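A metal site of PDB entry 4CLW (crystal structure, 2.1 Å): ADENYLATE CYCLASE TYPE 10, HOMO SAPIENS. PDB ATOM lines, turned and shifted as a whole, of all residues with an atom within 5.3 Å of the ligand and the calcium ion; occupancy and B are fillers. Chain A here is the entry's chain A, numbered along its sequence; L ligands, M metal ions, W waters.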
ATOM      1  N   ASP A  47     -16.635   0.837  13.374  1.00  0.00           N
ATOM      2  CA  ASP A  47     -16.318   1.895  14.361  1.00  0.00           C
ATOM      3  C   ASP A  47     -14.901   2.378  14.176  1.00  0.00           C
ATOM      4  O   ASP A  47     -13.969   1.604  14.276  1.00  0.00           O
ATOM      5  CB  ASP A  47     -16.494   1.379  15.804  1.00  0.00           C
ATOM      6  CG  ASP A  47     -16.219   2.462  16.882  1.00  0.00           C
ATOM      7  OD1 ASP A  47     -16.589   3.634  16.662  1.00  0.00           O
ATOM      8  OD2 ASP A  47     -15.613   2.137  17.951  1.00  0.00           O
ATOM      9  N   ILE A  48     -14.707   3.671  13.939  1.00  0.00           N
ATOM     10  CA  ILE A  48     -13.349   4.218  14.021  1.00  0.00           C
ATOM     11  C   ILE A  48     -12.962   4.753  15.402  1.00  0.00           C
ATOM     12  O   ILE A  48     -13.715   5.516  15.997  1.00  0.00           O
ATOM     13  CB  ILE A  48     -13.158   5.379  13.078  1.00  0.00           C
ATOM     14  CG1 ILE A  48     -13.324   4.857  11.647  1.00  0.00           C
ATOM     15  CG2 ILE A  48     -11.794   6.029  13.307  1.00  0.00           C
ATOM     16  CD1 ILE A  48     -13.245   5.956  10.622  1.00  0.00           C
ATOM     17  N   SER A  49     -11.770   4.398  15.850  1.00  0.00           N
ATOM     18  CA  SER A  49     -11.167   4.905  17.060  1.00  0.00           C
ATOM     19  C   SER A  49     -10.103   5.930  16.769  1.00  0.00           C
ATOM     20  O   SER A  49      -9.382   5.841  15.787  1.00  0.00           O
ATOM     21  CB  SER A  49     -10.489   3.771  17.855  1.00  0.00           C
ATOM     22  OG  SER A  49     -11.206   3.550  19.034  1.00  0.00           O
ATOM     23  N   GLY A  50      -9.991   6.895  17.671  1.00  0.00           N
ATOM     24  CA  GLY A  50      -8.953   7.910  17.601  1.00  0.00           C
ATOM     25  C   GLY A  50      -9.461   9.243  17.137  1.00  0.00           C
ATOM     26  O   GLY A  50      -8.756  10.216  17.237  1.00  0.00           O
ATOM     27  N   PHE A  51     -10.702   9.306  16.657  1.00  0.00           N
ATOM     28  CA  PHE A  51     -11.196  10.572  16.237  1.00  0.00           C
ATOM     29  C   PHE A  51     -11.600  11.525  17.299  1.00  0.00           C
ATOM     30  O   PHE A  51     -11.460  12.736  17.051  1.00  0.00           O
ATOM     31  CB  PHE A  51     -12.284  10.493  15.163  1.00  0.00           C
ATOM     32  CG  PHE A  51     -11.717  10.600  13.809  1.00  0.00           C
ATOM     33  CD1 PHE A  51     -11.169  11.813  13.373  1.00  0.00           C
ATOM     34  CD2 PHE A  51     -11.630   9.483  12.987  1.00  0.00           C
ATOM     35  CE1 PHE A  51     -10.571  11.908  12.116  1.00  0.00           C
ATOM     36  CE2 PHE A  51     -11.010   9.560  11.727  1.00  0.00           C
ATOM     37  CZ  PHE A  51     -10.484  10.770  11.285  1.00  0.00           C
ATOM     38  N   THR A  52     -12.097  11.073  18.454  1.00  0.00           N
ATOM     39  CA  THR A  52     -12.532  12.145  19.428  1.00  0.00           C
ATOM     40  C   THR A  52     -11.322  12.777  20.089  1.00  0.00           C
ATOM     41  O   THR A  52     -11.397  13.924  20.606  1.00  0.00           O
ATOM     42  CB  THR A  52     -13.519  11.668  20.531  1.00  0.00           C
ATOM     43  OG1 THR A  52     -12.857  10.668  21.333  1.00  0.00           O
ATOM     44  CG2 THR A  52     -14.779  11.073  19.887  1.00  0.00           C
ATOM     45  N   ALA A  53     -10.220  12.015  20.123  1.00  0.00           N
ATOM     46  CA  ALA A  53      -8.940  12.566  20.568  1.00  0.00           C
ATOM     47  C   ALA A  53      -8.406  13.561  19.538  1.00  0.00           C
ATOM     48  O   ALA A  53      -7.894  14.619  19.891  1.00  0.00           O
ATOM     49  CB  ALA A  53      -7.935  11.459  20.825  1.00  0.00           C
ATOM     50  N   ALA A  97     -22.955   7.517  13.077  1.00  0.00           N
ATOM     51  CA  ALA A  97     -23.072   7.907  14.507  1.00  0.00           C
ATOM     52  C   ALA A  97     -21.691   8.339  14.934  1.00  0.00           C
ATOM     53  O   ALA A  97     -20.808   7.521  15.221  1.00  0.00           O
ATOM     54  CB  ALA A  97     -23.586   6.740  15.321  1.00  0.00           C
ATOM     55  N   GLY A  98     -21.441   9.632  14.835  1.00  0.00           N
ATOM     56  CA  GLY A  98     -20.125  10.140  15.058  1.00  0.00           C
ATOM     57  C   GLY A  98     -19.142   9.635  14.022  1.00  0.00           C
ATOM     58  O   GLY A  98     -19.275   9.877  12.816  1.00  0.00           O
ATOM     59  N   ASP A  99     -18.116   8.953  14.505  1.00  0.00           N
ATOM     60  CA  ASP A  99     -17.081   8.372  13.637  1.00  0.00           C
ATOM     61  C   ASP A  99     -17.302   6.845  13.367  1.00  0.00           C
ATOM     62  O   ASP A  99     -16.362   6.145  13.056  1.00  0.00           O
ATOM     63  CB  ASP A  99     -15.692   8.652  14.266  1.00  0.00           C
ATOM     64  CG  ASP A  99     -15.592   8.160  15.712  1.00  0.00           C
ATOM     65  OD1 ASP A  99     -16.609   7.511  16.169  1.00  0.00           O
ATOM     66  OD2 ASP A  99     -14.556   8.533  16.395  1.00  0.00           O
ATOM     67  N   ALA A 100     -18.536   6.374  13.519  1.00  0.00           N
ATOM     68  CA  ALA A 100     -18.938   4.985  13.247  1.00  0.00           C
ATOM     69  C   ALA A 100     -20.115   4.986  12.251  1.00  0.00           C
ATOM     70  O   ALA A 100     -20.869   5.959  12.134  1.00  0.00           O
ATOM     71  CB  ALA A 100     -19.382   4.322  14.548  1.00  0.00           C
ATOM     72  N   LYS A 144     -12.664  -1.042  14.233  1.00  0.00           N
ATOM     73  CA  LYS A 144     -13.257  -2.280  14.707  1.00  0.00           C
ATOM     74  C   LYS A 144     -14.570  -2.512  13.927  1.00  0.00           C
ATOM     75  O   LYS A 144     -15.307  -1.558  13.702  1.00  0.00           O
ATOM     76  CB  LYS A 144     -13.578  -2.200  16.199  1.00  0.00           C
ATOM     77  CG  LYS A 144     -12.370  -1.976  17.097  1.00  0.00           C
ATOM     78  CD  LYS A 144     -12.734  -1.359  18.439  1.00  0.00           C
ATOM     79  CE  LYS A 144     -11.458  -0.813  19.094  1.00  0.00           C
ATOM     80  NZ  LYS A 144     -11.557  -0.614  20.562  1.00  0.00           N
ATOM     81  N   ARG A 176     -23.856  -4.676  17.767  1.00  0.00           N
ATOM     82  CA  ARG A 176     -23.188  -3.816  18.732  1.00  0.00           C
ATOM     83  C   ARG A 176     -22.339  -4.629  19.707  1.00  0.00           C
ATOM     84  O   ARG A 176     -21.229  -4.268  19.973  1.00  0.00           O
ATOM     85  CB  ARG A 176     -24.156  -2.919  19.523  1.00  0.00           C
ATOM     86  CG  ARG A 176     -23.408  -1.791  20.261  1.00  0.00           C
ATOM     87  CD  ARG A 176     -24.336  -0.660  20.757  1.00  0.00           C
ATOM     88  NE  ARG A 176     -24.872   0.123  19.649  1.00  0.00           N
ATOM     89  CZ  ARG A 176     -24.498   1.358  19.301  1.00  0.00           C
ATOM     90  NH1 ARG A 176     -23.573   2.011  20.011  1.00  0.00           N
ATOM     91  NH2 ARG A 176     -25.055   1.934  18.247  1.00  0.00           N
ATOM     92  N   PHE A 296     -28.310  13.249  26.216  1.00  0.00           N
ATOM     93  CA  PHE A 296     -28.409  11.907  25.729  1.00  0.00           C
ATOM     94  C   PHE A 296     -29.419  11.146  26.537  1.00  0.00           C
ATOM     95  O   PHE A 296     -29.227  10.860  27.765  1.00  0.00           O
ATOM     96  CB  PHE A 296     -27.022  11.249  25.806  1.00  0.00           C
ATOM     97  CG  PHE A 296     -26.605  10.535  24.566  1.00  0.00           C
ATOM     98  CD1 PHE A 296     -27.461   9.699  23.875  1.00  0.00           C
ATOM     99  CD2 PHE A 296     -25.323  10.716  24.064  1.00  0.00           C
ATOM    100  CE1 PHE A 296     -27.050   9.044  22.690  1.00  0.00           C
ATOM    101  CE2 PHE A 296     -24.891  10.084  22.893  1.00  0.00           C
ATOM    102  CZ  PHE A 296     -25.763   9.250  22.209  1.00  0.00           C
ATOM    103  N   ASN A 333     -30.528  15.039  17.229  1.00  0.00           N
ATOM    104  CA  ASN A 333     -29.525  14.871  16.197  1.00  0.00           C
ATOM    105  C   ASN A 333     -29.699  13.498  15.567  1.00  0.00           C
ATOM    106  O   ASN A 333     -29.600  13.365  14.371  1.00  0.00           O
ATOM    107  CB  ASN A 333     -28.105  15.025  16.744  1.00  0.00           C
ATOM    108  CG  ASN A 333     -27.028  14.729  15.692  1.00  0.00           C
ATOM    109  OD1 ASN A 333     -26.417  13.658  15.665  1.00  0.00           O
ATOM    110  ND2 ASN A 333     -26.791  15.681  14.831  1.00  0.00           N
ATOM    111  N   PHE A 336     -31.096   5.996  17.925  1.00  0.00           N
ATOM    112  CA  PHE A 336     -30.654   4.630  17.634  1.00  0.00           C
ATOM    113  C   PHE A 336     -30.802   3.721  18.808  1.00  0.00           C
ATOM    114  O   PHE A 336     -30.960   4.187  19.940  1.00  0.00           O
ATOM    115  CB  PHE A 336     -29.208   4.626  17.233  1.00  0.00           C
ATOM    116  CG  PHE A 336     -28.417   5.511  18.041  1.00  0.00           C
ATOM    117  CD1 PHE A 336     -27.908   5.085  19.250  1.00  0.00           C
ATOM    118  CD2 PHE A 336     -28.261   6.819  17.643  1.00  0.00           C
ATOM    119  CE1 PHE A 336     -27.183   5.947  20.057  1.00  0.00           C
ATOM    120  CE2 PHE A 336     -27.569   7.690  18.428  1.00  0.00           C
ATOM    121  CZ  PHE A 336     -27.025   7.250  19.634  1.00  0.00           C
ATOM    122  N   PHE A 338     -29.129   1.278  21.431  1.00  0.00           N
ATOM    123  CA  PHE A 338     -27.913   0.852  22.166  1.00  0.00           C
ATOM    124  C   PHE A 338     -28.078  -0.568  22.660  1.00  0.00           C
ATOM    125  O   PHE A 338     -29.140  -1.165  22.460  1.00  0.00           O
ATOM    126  CB  PHE A 338     -27.667   1.727  23.385  1.00  0.00           C
ATOM    127  CG  PHE A 338     -26.504   2.649  23.236  1.00  0.00           C
ATOM    128  CD1 PHE A 338     -26.345   3.433  22.103  1.00  0.00           C
ATOM    129  CD2 PHE A 338     -25.578   2.767  24.254  1.00  0.00           C
ATOM    130  CE1 PHE A 338     -25.263   4.302  21.977  1.00  0.00           C
ATOM    131  CE2 PHE A 338     -24.500   3.629  24.133  1.00  0.00           C
ATOM    132  CZ  PHE A 338     -24.344   4.400  22.998  1.00  0.00           C
ATOM    133  N   LEU A 345     -30.125  11.332  20.837  1.00  0.00           N
ATOM    134  CA  LEU A 345     -29.012  12.242  21.019  1.00  0.00           C
ATOM    135  C   LEU A 345     -29.479  13.641  20.709  1.00  0.00           C
ATOM    136  O   LEU A 345     -29.755  13.970  19.553  1.00  0.00           O
ATOM    137  CB  LEU A 345     -27.857  11.854  20.164  1.00  0.00           C
ATOM    138  CG  LEU A 345     -26.465  12.467  20.412  1.00  0.00           C
ATOM    139  CD1 LEU A 345     -25.490  11.919  19.387  1.00  0.00           C
ATOM    140  CD2 LEU A 345     -26.437  13.947  20.394  1.00  0.00           C
ATOM    141  N   THR A 405     -23.532  15.169  11.704  1.00  0.00           N
ATOM    142  CA  THR A 405     -23.245  14.447  12.953  1.00  0.00           C
ATOM    143  C   THR A 405     -22.433  15.297  13.996  1.00  0.00           C
ATOM    144  O   THR A 405     -21.952  16.390  13.685  1.00  0.00           O
ATOM    145  CB  THR A 405     -22.664  13.023  12.669  1.00  0.00           C
ATOM    146  OG1 THR A 405     -22.727  12.215  13.890  1.00  0.00           O
ATOM    147  CG2 THR A 405     -21.260  13.102  12.256  1.00  0.00           C
ATOM    148  N   VAL A 406     -22.362  14.796  15.220  1.00  0.00           N
ATOM    149  CA  VAL A 406     -21.570  15.417  16.267  1.00  0.00           C
ATOM    150  C   VAL A 406     -20.533  14.393  16.791  1.00  0.00           C
ATOM    151  O   VAL A 406     -20.817  13.219  16.919  1.00  0.00           O
ATOM    152  CB  VAL A 406     -22.425  15.935  17.396  1.00  0.00           C
ATOM    153  CG1 VAL A 406     -23.220  17.080  16.913  1.00  0.00           C
ATOM    154  CG2 VAL A 406     -23.356  14.827  17.953  1.00  0.00           C
ATOM    155  N   ILE A 407     -19.304  14.851  16.975  1.00  0.00           N
ATOM    156  CA  ILE A 407     -18.214  14.026  17.449  1.00  0.00           C
ATOM    157  C   ILE A 407     -17.514  14.828  18.527  1.00  0.00           C
ATOM    158  O   ILE A 407     -17.233  16.057  18.372  1.00  0.00           O
ATOM    159  CB  ILE A 407     -17.211  13.732  16.323  1.00  0.00           C
ATOM    160  CG1 ILE A 407     -17.887  12.971  15.226  1.00  0.00           C
ATOM    161  CG2 ILE A 407     -15.984  12.942  16.828  1.00  0.00           C
ATOM    162  CD1 ILE A 407     -17.030  12.832  13.979  1.00  0.00           C
ATOM    163  N   VAL A 411     -19.622  14.180  23.830  1.00  0.00           N
ATOM    164  CA  VAL A 411     -20.698  13.343  23.307  1.00  0.00           C
ATOM    165  C   VAL A 411     -20.517  11.950  23.903  1.00  0.00           C
ATOM    166  O   VAL A 411     -21.503  11.363  24.397  1.00  0.00           O
ATOM    167  CB  VAL A 411     -20.722  13.271  21.725  1.00  0.00           C
ATOM    168  CG1 VAL A 411     -21.853  12.437  21.268  1.00  0.00           C
ATOM    169  CG2 VAL A 411     -20.812  14.644  21.037  1.00  0.00           C
ATOM    170  N   ASN A 412     -19.284  11.426  23.861  1.00  0.00           N
ATOM    171  CA  ASN A 412     -18.976  10.142  24.481  1.00  0.00           C
ATOM    172  C   ASN A 412     -19.320  10.135  26.008  1.00  0.00           C
ATOM    173  O   ASN A 412     -19.863   9.164  26.540  1.00  0.00           O
ATOM    174  CB  ASN A 412     -17.463   9.807  24.395  1.00  0.00           C
ATOM    175  CG  ASN A 412     -16.973   9.509  22.982  1.00  0.00           C
ATOM    176  OD1 ASN A 412     -17.676   9.784  22.001  1.00  0.00           O
ATOM    177  ND2 ASN A 412     -15.771   8.948  22.878  1.00  0.00           N
ATOM    178  N   ALA A 415     -23.050   9.868  26.691  1.00  0.00           N
ATOM    179  CA  ALA A 415     -23.432   8.488  26.373  1.00  0.00           C
ATOM    180  C   ALA A 415     -23.025   7.495  27.455  1.00  0.00           C
ATOM    181  O   ALA A 415     -23.825   6.674  27.844  1.00  0.00           O
ATOM    182  CB  ALA A 415     -22.898   8.035  25.014  1.00  0.00           C
ATOM    183  N   ARG A 416     -21.804   7.617  27.990  1.00  0.00           N
ATOM    184  CA  ARG A 416     -21.376   6.739  29.052  1.00  0.00           C
ATOM    185  C   ARG A 416     -22.105   7.023  30.392  1.00  0.00           C
ATOM    186  O   ARG A 416     -22.358   6.080  31.150  1.00  0.00           O
ATOM    187  CB  ARG A 416     -19.864   6.799  29.287  1.00  0.00           C
ATOM    188  CG  ARG A 416     -18.996   6.497  28.047  1.00  0.00           C
ATOM    189  CD  ARG A 416     -19.396   5.165  27.497  1.00  0.00           C
ATOM    190  NE  ARG A 416     -18.415   4.498  26.654  1.00  0.00           N
ATOM    191  CZ  ARG A 416     -18.683   3.384  25.962  1.00  0.00           C
ATOM    192  NH1 ARG A 416     -19.892   2.805  26.013  1.00  0.00           N
ATOM    193  NH2 ARG A 416     -17.750   2.831  25.206  1.00  0.00           N
ATOM    194  N   MET A 419     -25.413   5.279  30.711  1.00  0.00           N
ATOM    195  CA  MET A 419     -25.201   3.829  30.862  1.00  0.00           C
ATOM    196  C   MET A 419     -24.658   3.512  32.236  1.00  0.00           C
ATOM    197  O   MET A 419     -25.063   2.568  32.852  1.00  0.00           O
ATOM    198  CB  MET A 419     -24.155   3.269  29.875  1.00  0.00           C
ATOM    199  CG  MET A 419     -24.574   3.252  28.413  1.00  0.00           C
ATOM    200  SD  MET A 419     -23.226   2.687  27.338  1.00  0.00           S
ATOM    201  CE  MET A 419     -22.697   4.260  26.676  1.00  0.00           C
ATOM    202  N   LYS A 451     -15.788   3.495  30.098  1.00  0.00           N
ATOM    203  CA  LYS A 451     -15.127   3.076  28.841  1.00  0.00           C
ATOM    204  C   LYS A 451     -14.854   4.214  27.893  1.00  0.00           C
ATOM    205  O   LYS A 451     -15.799   4.841  27.320  1.00  0.00           O
ATOM    206  CB  LYS A 451     -15.963   2.010  28.096  1.00  0.00           C
ATOM    207  N   GLY A 452     -13.572   4.456  27.697  1.00  0.00           N
ATOM    208  CA  GLY A 452     -13.150   5.444  26.720  1.00  0.00           C
ATOM    209  C   GLY A 452     -13.594   6.826  27.171  1.00  0.00           C
ATOM    210  O   GLY A 452     -14.225   7.597  26.407  1.00  0.00           O
HETATM  211  P1  LIG L   1     -13.431   7.555  19.773  1.00  0.00           P
HETATM  212  O1  LIG L   1     -14.704   7.474  18.942  1.00  0.00           O
HETATM  213  O2  LIG L   1     -12.197   8.194  19.112  1.00  0.00           O
HETATM  214  O3  LIG L   1     -13.805   8.248  21.050  1.00  0.00           O
HETATM  215  P2  LIG L   1     -13.986   4.826  20.477  1.00  0.00           P
HETATM  216  O4  LIG L   1     -14.595   4.271  19.255  1.00  0.00           O
HETATM  217  O5  LIG L   1     -13.022   3.641  21.004  1.00  0.00           O
HETATM  218  O6  LIG L   1     -12.971   6.028  20.019  1.00  0.00           O
HETATM  219  P3  LIG L   1     -16.564   4.215  22.141  1.00  0.00           P
HETATM  220  O7  LIG L   1     -15.885   2.898  22.726  1.00  0.00           O
HETATM  221  O8  LIG L   1     -17.491   3.886  21.013  1.00  0.00           O
HETATM  222  C1  LIG L   1     -15.239   5.407  21.675  1.00  0.00           C
HETATM  223  O9  LIG L   1     -17.451   4.956  23.283  1.00  0.00           O
HETATM  224  C2  LIG L   1     -18.163   6.133  22.930  1.00  0.00           C
HETATM  225  C3  LIG L   1     -19.651   5.967  23.135  1.00  0.00           C
HETATM  226  O10 LIG L   1     -20.264   7.203  22.789  1.00  0.00           O
HETATM  227  C4  LIG L   1     -20.310   4.896  22.270  1.00  0.00           C
HETATM  228  O11 LIG L   1     -21.279   4.256  23.088  1.00  0.00           O
HETATM  229  C5  LIG L   1     -21.056   5.637  21.184  1.00  0.00           C
HETATM  230  O12 LIG L   1     -22.300   5.015  20.839  1.00  0.00           O
HETATM  231  C6  LIG L   1     -21.315   7.007  21.833  1.00  0.00           C
HETATM  232  N1  LIG L   1     -21.332   8.082  20.812  1.00  0.00           N
HETATM  233  C7  LIG L   1     -20.397   9.036  20.649  1.00  0.00           C
HETATM  234  N2  LIG L   1     -20.701   9.856  19.617  1.00  0.00           N
HETATM  235  C8  LIG L   1     -21.875   9.435  19.123  1.00  0.00           C
HETATM  236  C9  LIG L   1     -22.767   9.861  18.009  1.00  0.00           C
HETATM  237  N3  LIG L   1     -22.482  10.948  17.264  1.00  0.00           N
HETATM  238  N4  LIG L   1     -23.906   9.160  17.826  1.00  0.00           N
HETATM  239  C10 LIG L   1     -24.231   8.078  18.596  1.00  0.00           C
HETATM  240  N5  LIG L   1     -23.469   7.625  19.616  1.00  0.00           N
HETATM  241  C11 LIG L   1     -22.298   8.268  19.912  1.00  0.00           C
HETATM  242 CA    CA M   1     -15.757   5.730  17.597  1.00  0.00          CA
HETATM  243  O   HOH W   1     -20.573   6.331  17.690  1.00  0.00           O
HETATM  244  O   HOH W   2     -17.022   8.240  19.631  1.00  0.00           O
HETATM  245  O   HOH W   3     -17.883   5.786  18.753  1.00  0.00           O
HETATM  246  O   HOH W   4     -18.108   9.513  17.499  1.00  0.00           O
HETATM  247  O   HOH W   5     -18.107  11.427  19.708  1.00  0.00           O
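N of Thr 52 lies within hydrogen-bond range of O2 of the ligand, at 3.0 Å.
An oxygen (O7) of the ligand lies within salt-bridge range of the guanidinium group of Arg 416 (3.1 Å).
An oxygen (O2) of the ligand is in hydrogen-bond range of the backbone NH (N) of Gly 50, 2.9 Å away.
O3 of the ligand lies within hydrogen-bond range of ND2 of Asn 412.
O3 of the ligand lies within hydrogen-bond range of OG1 of Thr 52, at 2.6 Å.
O2 of the ligand is in hydrogen-bond range of N of Phe 51 (3.1 Å).
OG of Ser 49 lies within hydrogen-bond range of O5 of the ligand (2.7 Å).
O of Val 406 lies within hydrogen-bond range of N3 of the ligand (2.8 Å).
The guanidinium group of Arg 176 sits at hydrogen-bond distance from an oxygen (O12) of the ligand (3.4 Å).
O of Leu 345 is in hydrogen-bond range of N of Asn 333, at 2.7 Å.
NH1 of Arg 416 sits close to SD of Met 419, 3.6 Å away.
The backbone NH (N) of Asp 47 sits at hydrogen-bond distance from the backbone carbonyl oxygen (O) of Lys 144 (2.8 Å).
The guanidinium group (NE) of Arg 416 lies within hydrogen-bond range of the backbone carbonyl oxygen (O) of Lys 451, 2.7 Å away.
OG1 of Thr 405 sits at hydrogen-bond distance from N of Gly 98, at 3.0 Å.
A nitrogen (N3) of the ligand lies close to the backbone NH (N) of Gly 98, 3.0 Å away.
Merely in contact with the ligand: Ala 97 (3.5 Å), Phe 296 (3.8 Å), Phe 336 (3.1 Å), Phe 338 (3.0 Å), Leu 345 (3.5 Å), Thr 405 (3.6 Å), Val 411 (3.3 Å), Ala 415 (3.5 Å) and Met 419 (3.9 Å).
Within 4 Å of the ligand: Asp 47, Ile 48, Ser 49, Gly 50, Phe 51, Thr 52, Ala 97, Gly 98, Asp 99, Arg 176, Phe 296, Phe 336, Phe 338, Leu 345, Thr 405, Val 406, Val 411, Asn 412, Ala 415, Arg 416 and Met 419.
Three residues have an atom within 4 Å of the calcium ion: Asp 47, Ile 48 and Asp 99.
Water W3 binds the calcium ion (2.4 Å).
OD1 of Asp 99 is bound to the calcium ion (2.4 Å).
An oxygen (O1) of the ligand binds the calcium ion (2.4 Å).
OD1 of Asp 47 is bound to the calcium ion (2.4 Å).
O4 of the ligand binds the calcium ion, at 2.5 Å.
O of Ile 48 binds the calcium ion (2.6 Å).
Water W5 bridges the side-chain amide oxygen (OD1) of Asn 412 (2.9 Å) and a nitrogen (N2) of the ligand (3.0 Å).
Water W4 bridges N of Asp 99 (3.0 Å) and N2 of the ligand (3.4 Å).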
